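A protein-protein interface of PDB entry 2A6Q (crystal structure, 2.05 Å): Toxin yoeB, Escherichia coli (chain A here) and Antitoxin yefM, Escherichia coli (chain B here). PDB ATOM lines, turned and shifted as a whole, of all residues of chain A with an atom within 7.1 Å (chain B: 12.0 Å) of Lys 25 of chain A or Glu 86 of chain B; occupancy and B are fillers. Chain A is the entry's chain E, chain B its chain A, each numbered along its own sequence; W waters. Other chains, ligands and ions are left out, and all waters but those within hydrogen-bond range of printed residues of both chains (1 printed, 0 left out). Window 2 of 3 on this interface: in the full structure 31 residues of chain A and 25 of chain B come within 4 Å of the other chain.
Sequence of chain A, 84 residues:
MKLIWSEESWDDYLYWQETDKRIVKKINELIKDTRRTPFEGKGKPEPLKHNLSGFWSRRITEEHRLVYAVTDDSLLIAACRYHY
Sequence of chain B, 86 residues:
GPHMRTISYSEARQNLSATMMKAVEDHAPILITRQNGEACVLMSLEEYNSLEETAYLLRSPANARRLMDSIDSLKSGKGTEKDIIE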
ATOM      1  N   TYR A  13       4.706  22.520  22.636  1.00  0.00           N
ATOM      2  CA  TYR A  13       5.347  23.588  21.877  1.00  0.00           C
ATOM      3  C   TYR A  13       6.686  24.038  22.453  1.00  0.00           C
ATOM      4  O   TYR A  13       7.657  24.226  21.712  1.00  0.00           O
ATOM      5  CB  TYR A  13       4.401  24.785  21.784  1.00  0.00           C
ATOM      6  CG  TYR A  13       4.825  25.832  20.781  1.00  0.00           C
ATOM      7  CD1 TYR A  13       4.940  25.522  19.426  1.00  0.00           C
ATOM      8  CD2 TYR A  13       5.101  27.139  21.182  1.00  0.00           C
ATOM      9  CE1 TYR A  13       5.318  26.486  18.495  1.00  0.00           C
ATOM     10  CE2 TYR A  13       5.481  28.111  20.257  1.00  0.00           C
ATOM     11  CZ  TYR A  13       5.587  27.776  18.919  1.00  0.00           C
ATOM     12  OH  TYR A  13       5.966  28.729  18.009  1.00  0.00           O
ATOM     13  N   GLN A  17      10.619  23.815  21.375  1.00  0.00           N
ATOM     14  CA  GLN A  17      11.334  25.080  21.428  1.00  0.00           C
ATOM     15  C   GLN A  17      12.731  24.890  22.005  1.00  0.00           C
ATOM     16  O   GLN A  17      13.692  25.503  21.542  1.00  0.00           O
ATOM     17  CB  GLN A  17      10.542  26.075  22.276  1.00  0.00           C
ATOM     18  CG  GLN A  17      10.704  27.521  21.861  1.00  0.00           C
ATOM     19  CD  GLN A  17      10.627  27.702  20.359  1.00  0.00           C
ATOM     20  OE1 GLN A  17      11.607  27.487  19.653  1.00  0.00           O
ATOM     21  NE2 GLN A  17       9.455  28.082  19.861  1.00  0.00           N
ATOM     22  N   ASP A  20      14.112  20.799  19.478  1.00  0.00           N
ATOM     23  CA  ASP A  20      14.385  20.732  18.048  1.00  0.00           C
ATOM     24  C   ASP A  20      13.742  21.918  17.341  1.00  0.00           C
ATOM     25  O   ASP A  20      12.542  21.911  17.056  1.00  0.00           O
ATOM     26  CB  ASP A  20      13.837  19.426  17.467  1.00  0.00           C
ATOM     27  CG  ASP A  20      14.319  19.167  16.048  1.00  0.00           C
ATOM     28  OD1 ASP A  20      14.711  20.136  15.360  1.00  0.00           O
ATOM     29  OD2 ASP A  20      14.292  17.994  15.617  1.00  0.00           O
ATOM     30  N   LYS A  21      14.552  22.932  17.056  1.00  0.00           N
ATOM     31  CA  LYS A  21      14.072  24.133  16.393  1.00  0.00           C
ATOM     32  C   LYS A  21      13.527  23.836  15.001  1.00  0.00           C
ATOM     33  O   LYS A  21      12.684  24.573  14.486  1.00  0.00           O
ATOM     34  CB  LYS A  21      15.199  25.164  16.300  1.00  0.00           C
ATOM     35  CG  LYS A  21      14.736  26.540  15.848  1.00  0.00           C
ATOM     36  CD  LYS A  21      13.742  27.132  16.839  1.00  0.00           C
ATOM     37  CE  LYS A  21      13.185  28.458  16.348  1.00  0.00           C
ATOM     38  NZ  LYS A  21      12.167  29.006  17.290  1.00  0.00           N
ATOM     39  N   ARG A  22      14.011  22.761  14.389  1.00  0.00           N
ATOM     40  CA  ARG A  22      13.552  22.379  13.056  1.00  0.00           C
ATOM     41  C   ARG A  22      12.054  22.073  13.100  1.00  0.00           C
ATOM     42  O   ARG A  22      11.299  22.454  12.202  1.00  0.00           O
ATOM     43  CB  ARG A  22      14.326  21.149  12.566  1.00  0.00           C
ATOM     44  CG  ARG A  22      13.974  20.713  11.147  1.00  0.00           C
ATOM     45  CD  ARG A  22      14.844  19.549  10.680  1.00  0.00           C
ATOM     46  NE  ARG A  22      14.604  18.320  11.435  1.00  0.00           N
ATOM     47  CZ  ARG A  22      13.480  17.608  11.382  1.00  0.00           C
ATOM     48  NH1 ARG A  22      12.474  17.994  10.606  1.00  0.00           N
ATOM     49  NH2 ARG A  22      13.360  16.502  12.104  1.00  0.00           N
ATOM     50  N   ILE A  23      11.633  21.386  14.158  1.00  0.00           N
ATOM     51  CA  ILE A  23      10.235  21.026  14.343  1.00  0.00           C
ATOM     52  C   ILE A  23       9.408  22.267  14.656  1.00  0.00           C
ATOM     53  O   ILE A  23       8.232  22.347  14.298  1.00  0.00           O
ATOM     54  CB  ILE A  23      10.077  20.016  15.493  1.00  0.00           C
ATOM     55  CG1 ILE A  23      10.865  18.746  15.173  1.00  0.00           C
ATOM     56  CG2 ILE A  23       8.605  19.698  15.713  1.00  0.00           C
ATOM     57  CD1 ILE A  23      10.456  18.081  13.870  1.00  0.00           C
ATOM     58  N   VAL A  24      10.029  23.230  15.331  1.00  0.00           N
ATOM     59  CA  VAL A  24       9.351  24.470  15.686  1.00  0.00           C
ATOM     60  C   VAL A  24       8.910  25.182  14.419  1.00  0.00           C
ATOM     61  O   VAL A  24       7.748  25.566  14.280  1.00  0.00           O
ATOM     62  CB  VAL A  24      10.280  25.406  16.493  1.00  0.00           C
ATOM     63  CG1 VAL A  24       9.573  26.725  16.791  1.00  0.00           C
ATOM     64  CG2 VAL A  24      10.691  24.729  17.786  1.00  0.00           C
ATOM     65  N   LYS A  25       9.842  25.339  13.487  1.00  0.00           N
ATOM     66  CA  LYS A  25       9.559  26.006  12.229  1.00  0.00           C
ATOM     67  C   LYS A  25       8.435  25.327  11.462  1.00  0.00           C
ATOM     68  O   LYS A  25       7.636  25.992  10.806  1.00  0.00           O
ATOM     69  CB  LYS A  25      10.819  26.057  11.362  1.00  0.00           C
ATOM     70  CG  LYS A  25      11.935  26.904  11.953  1.00  0.00           C
ATOM     71  CD  LYS A  25      11.476  28.345  12.149  1.00  0.00           C
ATOM     72  CE  LYS A  25      12.581  29.218  12.724  1.00  0.00           C
ATOM     73  NZ  LYS A  25      12.112  30.615  12.942  1.00  0.00           N
ATOM     74  N   LYS A  26       8.372  24.002  11.541  1.00  0.00           N
ATOM     75  CA  LYS A  26       7.325  23.267  10.842  1.00  0.00           C
ATOM     76  C   LYS A  26       5.972  23.594  11.467  1.00  0.00           C
ATOM     77  O   LYS A  26       4.994  23.842  10.763  1.00  0.00           O
ATOM     78  CB  LYS A  26       7.591  21.757  10.915  1.00  0.00           C
ATOM     79  CG  LYS A  26       8.969  21.348  10.397  1.00  0.00           C
ATOM     80  CD  LYS A  26       9.162  19.834  10.403  1.00  0.00           C
ATOM     81  CE  LYS A  26       8.275  19.150   9.375  1.00  0.00           C
ATOM     82  NZ  LYS A  26       8.588  19.558   7.977  1.00  0.00           N
ATOM     83  N   ILE A  27       5.928  23.599  12.795  1.00  0.00           N
ATOM     84  CA  ILE A  27       4.700  23.904  13.519  1.00  0.00           C
ATOM     85  C   ILE A  27       4.215  25.311  13.172  1.00  0.00           C
ATOM     86  O   ILE A  27       3.036  25.512  12.887  1.00  0.00           O
ATOM     87  CB  ILE A  27       4.909  23.784  15.055  1.00  0.00           C
ATOM     88  CG1 ILE A  27       5.195  22.324  15.422  1.00  0.00           C
ATOM     89  CG2 ILE A  27       3.664  24.282  15.804  1.00  0.00           C
ATOM     90  CD1 ILE A  27       5.507  22.100  16.885  1.00  0.00           C
ATOM     91  N   ASN A  28       5.126  26.282  13.183  1.00  0.00           N
ATOM     92  CA  ASN A  28       4.762  27.662  12.860  1.00  0.00           C
ATOM     93  C   ASN A  28       4.208  27.781  11.445  1.00  0.00           C
ATOM     94  O   ASN A  28       3.250  28.518  11.209  1.00  0.00           O
ATOM     95  CB  ASN A  28       5.965  28.600  13.019  1.00  0.00           C
ATOM     96  CG  ASN A  28       6.433  28.715  14.461  1.00  0.00           C
ATOM     97  OD1 ASN A  28       5.631  28.659  15.390  1.00  0.00           O
ATOM     98  ND2 ASN A  28       7.736  28.894  14.653  1.00  0.00           N
ATOM     99  N   GLU A  29       4.810  27.059  10.503  1.00  0.00           N
ATOM    100  CA  GLU A  29       4.353  27.091   9.115  1.00  0.00           C
ATOM    101  C   GLU A  29       2.932  26.557   9.023  1.00  0.00           C
ATOM    102  O   GLU A  29       2.091  27.107   8.308  1.00  0.00           O
ATOM    103  CB  GLU A  29       5.268  26.245   8.222  1.00  0.00           C
ATOM    104  CG  GLU A  29       6.713  26.721   8.169  1.00  0.00           C
ATOM    105  CD  GLU A  29       6.833  28.185   7.784  1.00  0.00           C
ATOM    106  OE1 GLU A  29       6.323  28.562   6.704  1.00  0.00           O
ATOM    107  OE2 GLU A  29       7.440  28.958   8.562  1.00  0.00           O
ATOM    108  N   LEU A  30       2.670  25.476   9.748  1.00  0.00           N
ATOM    109  CA  LEU A  30       1.346  24.873   9.752  1.00  0.00           C
ATOM    110  C   LEU A  30       0.315  25.807  10.382  1.00  0.00           C
ATOM    111  O   LEU A  30      -0.801  25.942   9.879  1.00  0.00           O
ATOM    112  CB  LEU A  30       1.376  23.547  10.511  1.00  0.00           C
ATOM    113  CG  LEU A  30       2.222  22.451   9.860  1.00  0.00           C
ATOM    114  CD1 LEU A  30       2.132  21.181  10.697  1.00  0.00           C
ATOM    115  CD2 LEU A  30       1.725  22.197   8.445  1.00  0.00           C
ATOM    116  N   ILE A  31       0.691  26.435  11.492  1.00  0.00           N
ATOM    117  CA  ILE A  31      -0.201  27.364  12.180  1.00  0.00           C
ATOM    118  C   ILE A  31      -0.508  28.549  11.269  1.00  0.00           C
ATOM    119  O   ILE A  31      -1.658  28.956  11.133  1.00  0.00           O
ATOM    120  CB  ILE A  31       0.430  27.876  13.498  1.00  0.00           C
ATOM    121  CG1 ILE A  31       0.468  26.741  14.525  1.00  0.00           C
ATOM    122  CG2 ILE A  31      -0.359  29.071  14.029  1.00  0.00           C
ATOM    123  CD1 ILE A  31       1.063  27.125  15.867  1.00  0.00           C
ATOM    124  N   LYS A  32       0.524  29.093  10.638  1.00  0.00           N
ATOM    125  CA  LYS A  32       0.338  30.218   9.736  1.00  0.00           C
ATOM    126  C   LYS A  32      -0.538  29.839   8.546  1.00  0.00           C
ATOM    127  O   LYS A  32      -1.319  30.654   8.055  1.00  0.00           O
ATOM    128  CB  LYS A  32       1.698  30.729   9.252  1.00  0.00           C
ATOM    129  CG  LYS A  32       2.505  31.405  10.353  1.00  0.00           C
ATOM    130  CD  LYS A  32       3.882  31.856   9.881  1.00  0.00           C
ATOM    131  CE  LYS A  32       4.808  30.676   9.624  1.00  0.00           C
ATOM    132  NZ  LYS A  32       6.193  31.130   9.319  1.00  0.00           N
ATOM    133  N   LYS B  82      -1.452  32.677  23.444  1.00  0.00           N
ATOM    134  CA  LYS B  82      -0.013  32.910  23.343  1.00  0.00           C
ATOM    135  C   LYS B  82       0.358  32.981  21.867  1.00  0.00           C
ATOM    136  O   LYS B  82      -0.247  32.300  21.038  1.00  0.00           O
ATOM    137  CB  LYS B  82       0.765  31.768  24.005  1.00  0.00           C
ATOM    138  CG  LYS B  82       0.693  31.724  25.527  1.00  0.00           C
ATOM    139  CD  LYS B  82       1.560  32.805  26.152  1.00  0.00           C
ATOM    140  CE  LYS B  82       1.640  32.648  27.664  1.00  0.00           C
ATOM    141  NZ  LYS B  82       2.563  33.642  28.289  1.00  0.00           N
ATOM    142  N   ASP B  83       1.346  33.803  21.533  1.00  0.00           N
ATOM    143  CA  ASP B  83       1.764  33.919  20.144  1.00  0.00           C
ATOM    144  C   ASP B  83       2.894  32.939  19.869  1.00  0.00           C
ATOM    145  O   ASP B  83       3.498  32.402  20.796  1.00  0.00           O
ATOM    146  CB  ASP B  83       2.236  35.338  19.835  1.00  0.00           C
ATOM    147  CG  ASP B  83       2.323  35.606  18.343  1.00  0.00           C
ATOM    148  OD1 ASP B  83       3.042  36.548  17.949  1.00  0.00           O
ATOM    149  OD2 ASP B  83       1.666  34.880  17.566  1.00  0.00           O
ATOM    150  N   ILE B  84       3.182  32.713  18.591  1.00  0.00           N
ATOM    151  CA  ILE B  84       4.237  31.783  18.204  1.00  0.00           C
ATOM    152  C   ILE B  84       5.627  32.336  18.481  1.00  0.00           C
ATOM    153  O   ILE B  84       5.921  33.492  18.177  1.00  0.00           O
ATOM    154  CB  ILE B  84       4.148  31.419  16.704  1.00  0.00           C
ATOM    155  CG1 ILE B  84       4.346  32.668  15.845  1.00  0.00           C
ATOM    156  CG2 ILE B  84       2.800  30.789  16.405  1.00  0.00           C
ATOM    157  CD1 ILE B  84       4.408  32.384  14.361  1.00  0.00           C
ATOM    158  N   ILE B  85       6.478  31.501  19.069  1.00  0.00           N
ATOM    159  CA  ILE B  85       7.847  31.894  19.372  1.00  0.00           C
ATOM    160  C   ILE B  85       8.660  31.729  18.096  1.00  0.00           C
ATOM    161  O   ILE B  85       9.159  30.644  17.798  1.00  0.00           O
ATOM    162  CB  ILE B  85       8.456  31.010  20.482  1.00  0.00           C
ATOM    163  CG1 ILE B  85       7.591  31.085  21.744  1.00  0.00           C
ATOM    164  CG2 ILE B  85       9.875  31.461  20.789  1.00  0.00           C
ATOM    165  CD1 ILE B  85       7.412  32.484  22.292  1.00  0.00           C
ATOM    166  N   GLU B  86       8.775  32.815  17.340  1.00  0.00           N
ATOM    167  CA  GLU B  86       9.508  32.812  16.082  1.00  0.00           C
ATOM    168  C   GLU B  86      10.966  32.408  16.277  1.00  0.00           C
ATOM    169  O   GLU B  86      11.375  32.215  17.441  1.00  0.00           O
ATOM    170  CB  GLU B  86       9.444  34.198  15.445  1.00  0.00           C
ATOM    171  CG  GLU B  86       9.813  34.206  13.982  1.00  0.00           C
ATOM    172  CD  GLU B  86       8.879  33.350  13.160  1.00  0.00           C
ATOM    173  OE1 GLU B  86       7.668  33.656  13.127  1.00  0.00           O
ATOM    174  OE2 GLU B  86       9.354  32.369  12.550  1.00  0.00           O
ATOM    175  OXT GLU B  86      11.682  32.294  15.261  1.00  0.00           O
HETATM  176  O   HOH W   1       8.726  29.757  12.390  1.00  0.00           O
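The backbone NH (N) of Ile 85 of chain B lies within hydrogen-bond range of the side-chain hydroxyl (OH) of Tyr 13 of chain A, 3.0 Å away. The backbone carbonyl oxygen (O) of Ile 85 of chain B lies close to the side-chain amide nitrogen (NE2) of Gln 17 of chain A (3.3 Å). NZ of Lys 21 of chain A lies within hydrogen-bond range of O of Ile 85 of chain B. The chain-end carboxylate of Glu 86 of chain B is in salt-bridge range of the side-chain amino group of Lys 21 of chain A. The chain-end carboxylate (OXT) of Glu 86 of chain B lies within salt-bridge range of the side-chain amino group (NZ) of Lys 25 of chain A.
The side-chain hydroxyl (OH) of Tyr 13 of chain A is in hydrogen-bond range of the side-chain amide oxygen (OD1) of Asn 28 of chain A. NZ of Lys 21 of chain A sits at hydrogen-bond distance from OE1 of Gln 17 of chain A, at 2.9 Å. O of Val 24 of chain A is in hydrogen-bond range of ND2 of Asn 28 of chain A (3.3 Å).
Among the printed residues, pairs that only touch across the chains: Asn 28 of chain A with Ile 84 of chain B, Tyr 13 of chain A with Ile 84 of chain B and Asn 28 of chain A with Ile 85 of chain B.
Lys 25 of chain A touches just one residue of chain B: Glu 86 (2.9 Å). Glu 86 of chain B touches two residues of chain A. Of chain B, only Ile 85 and Glu 86 come within 4 Å of Lys 21 of chain A. No residue of chain B comes within 4 Å of Val 24 of chain A. No residue of chain B comes within 4 Å of Ile 27 of chain A. Asn 28 of chain A touches just these residues of chain B: Ile 84 and Ile 85. Glu 29 of chain A touches none of the printed residues of chain B. Printed residues of chain B within 4 Å of Tyr 13 of chain A: Ile 84 (3.5 Å) and Ile 85 (3.0 Å). Printed residues of chain B within 4 Å of Gln 17 of chain A: Ile 85. Of the printed residues of chain A, Ile 84 of chain B touches Tyr 13 and Asn 28. Lys 32 of chain A touches none of the printed residues of chain B. Asp 83 of chain B touches none of the printed residues of chain A. The nearest residue of chain B that does not touch Lys 25 of chain A is Ile 85 of chain B (5.7 Å). The nearest printed residue of chain A that does not touch Ile 85 of chain B is Val 24 of chain A (4.1 Å).
Along chain B the printed residues that touch a printed residue of chain A span positions 84 to 86. Among the printed residues, Asp or Glu carboxylates within 4 Å of a Lys or Arg side-chain nitrogen of the other chain: Lys 25 of chain A with Glu 86 of chain B (3.3 Å).
Water W1 lies within hydrogen-bond range of the side-chain amide nitrogen (ND2) of Asn 28 of chain A and the side-chain carboxylate (OE2) of Glu 86 of chain B.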
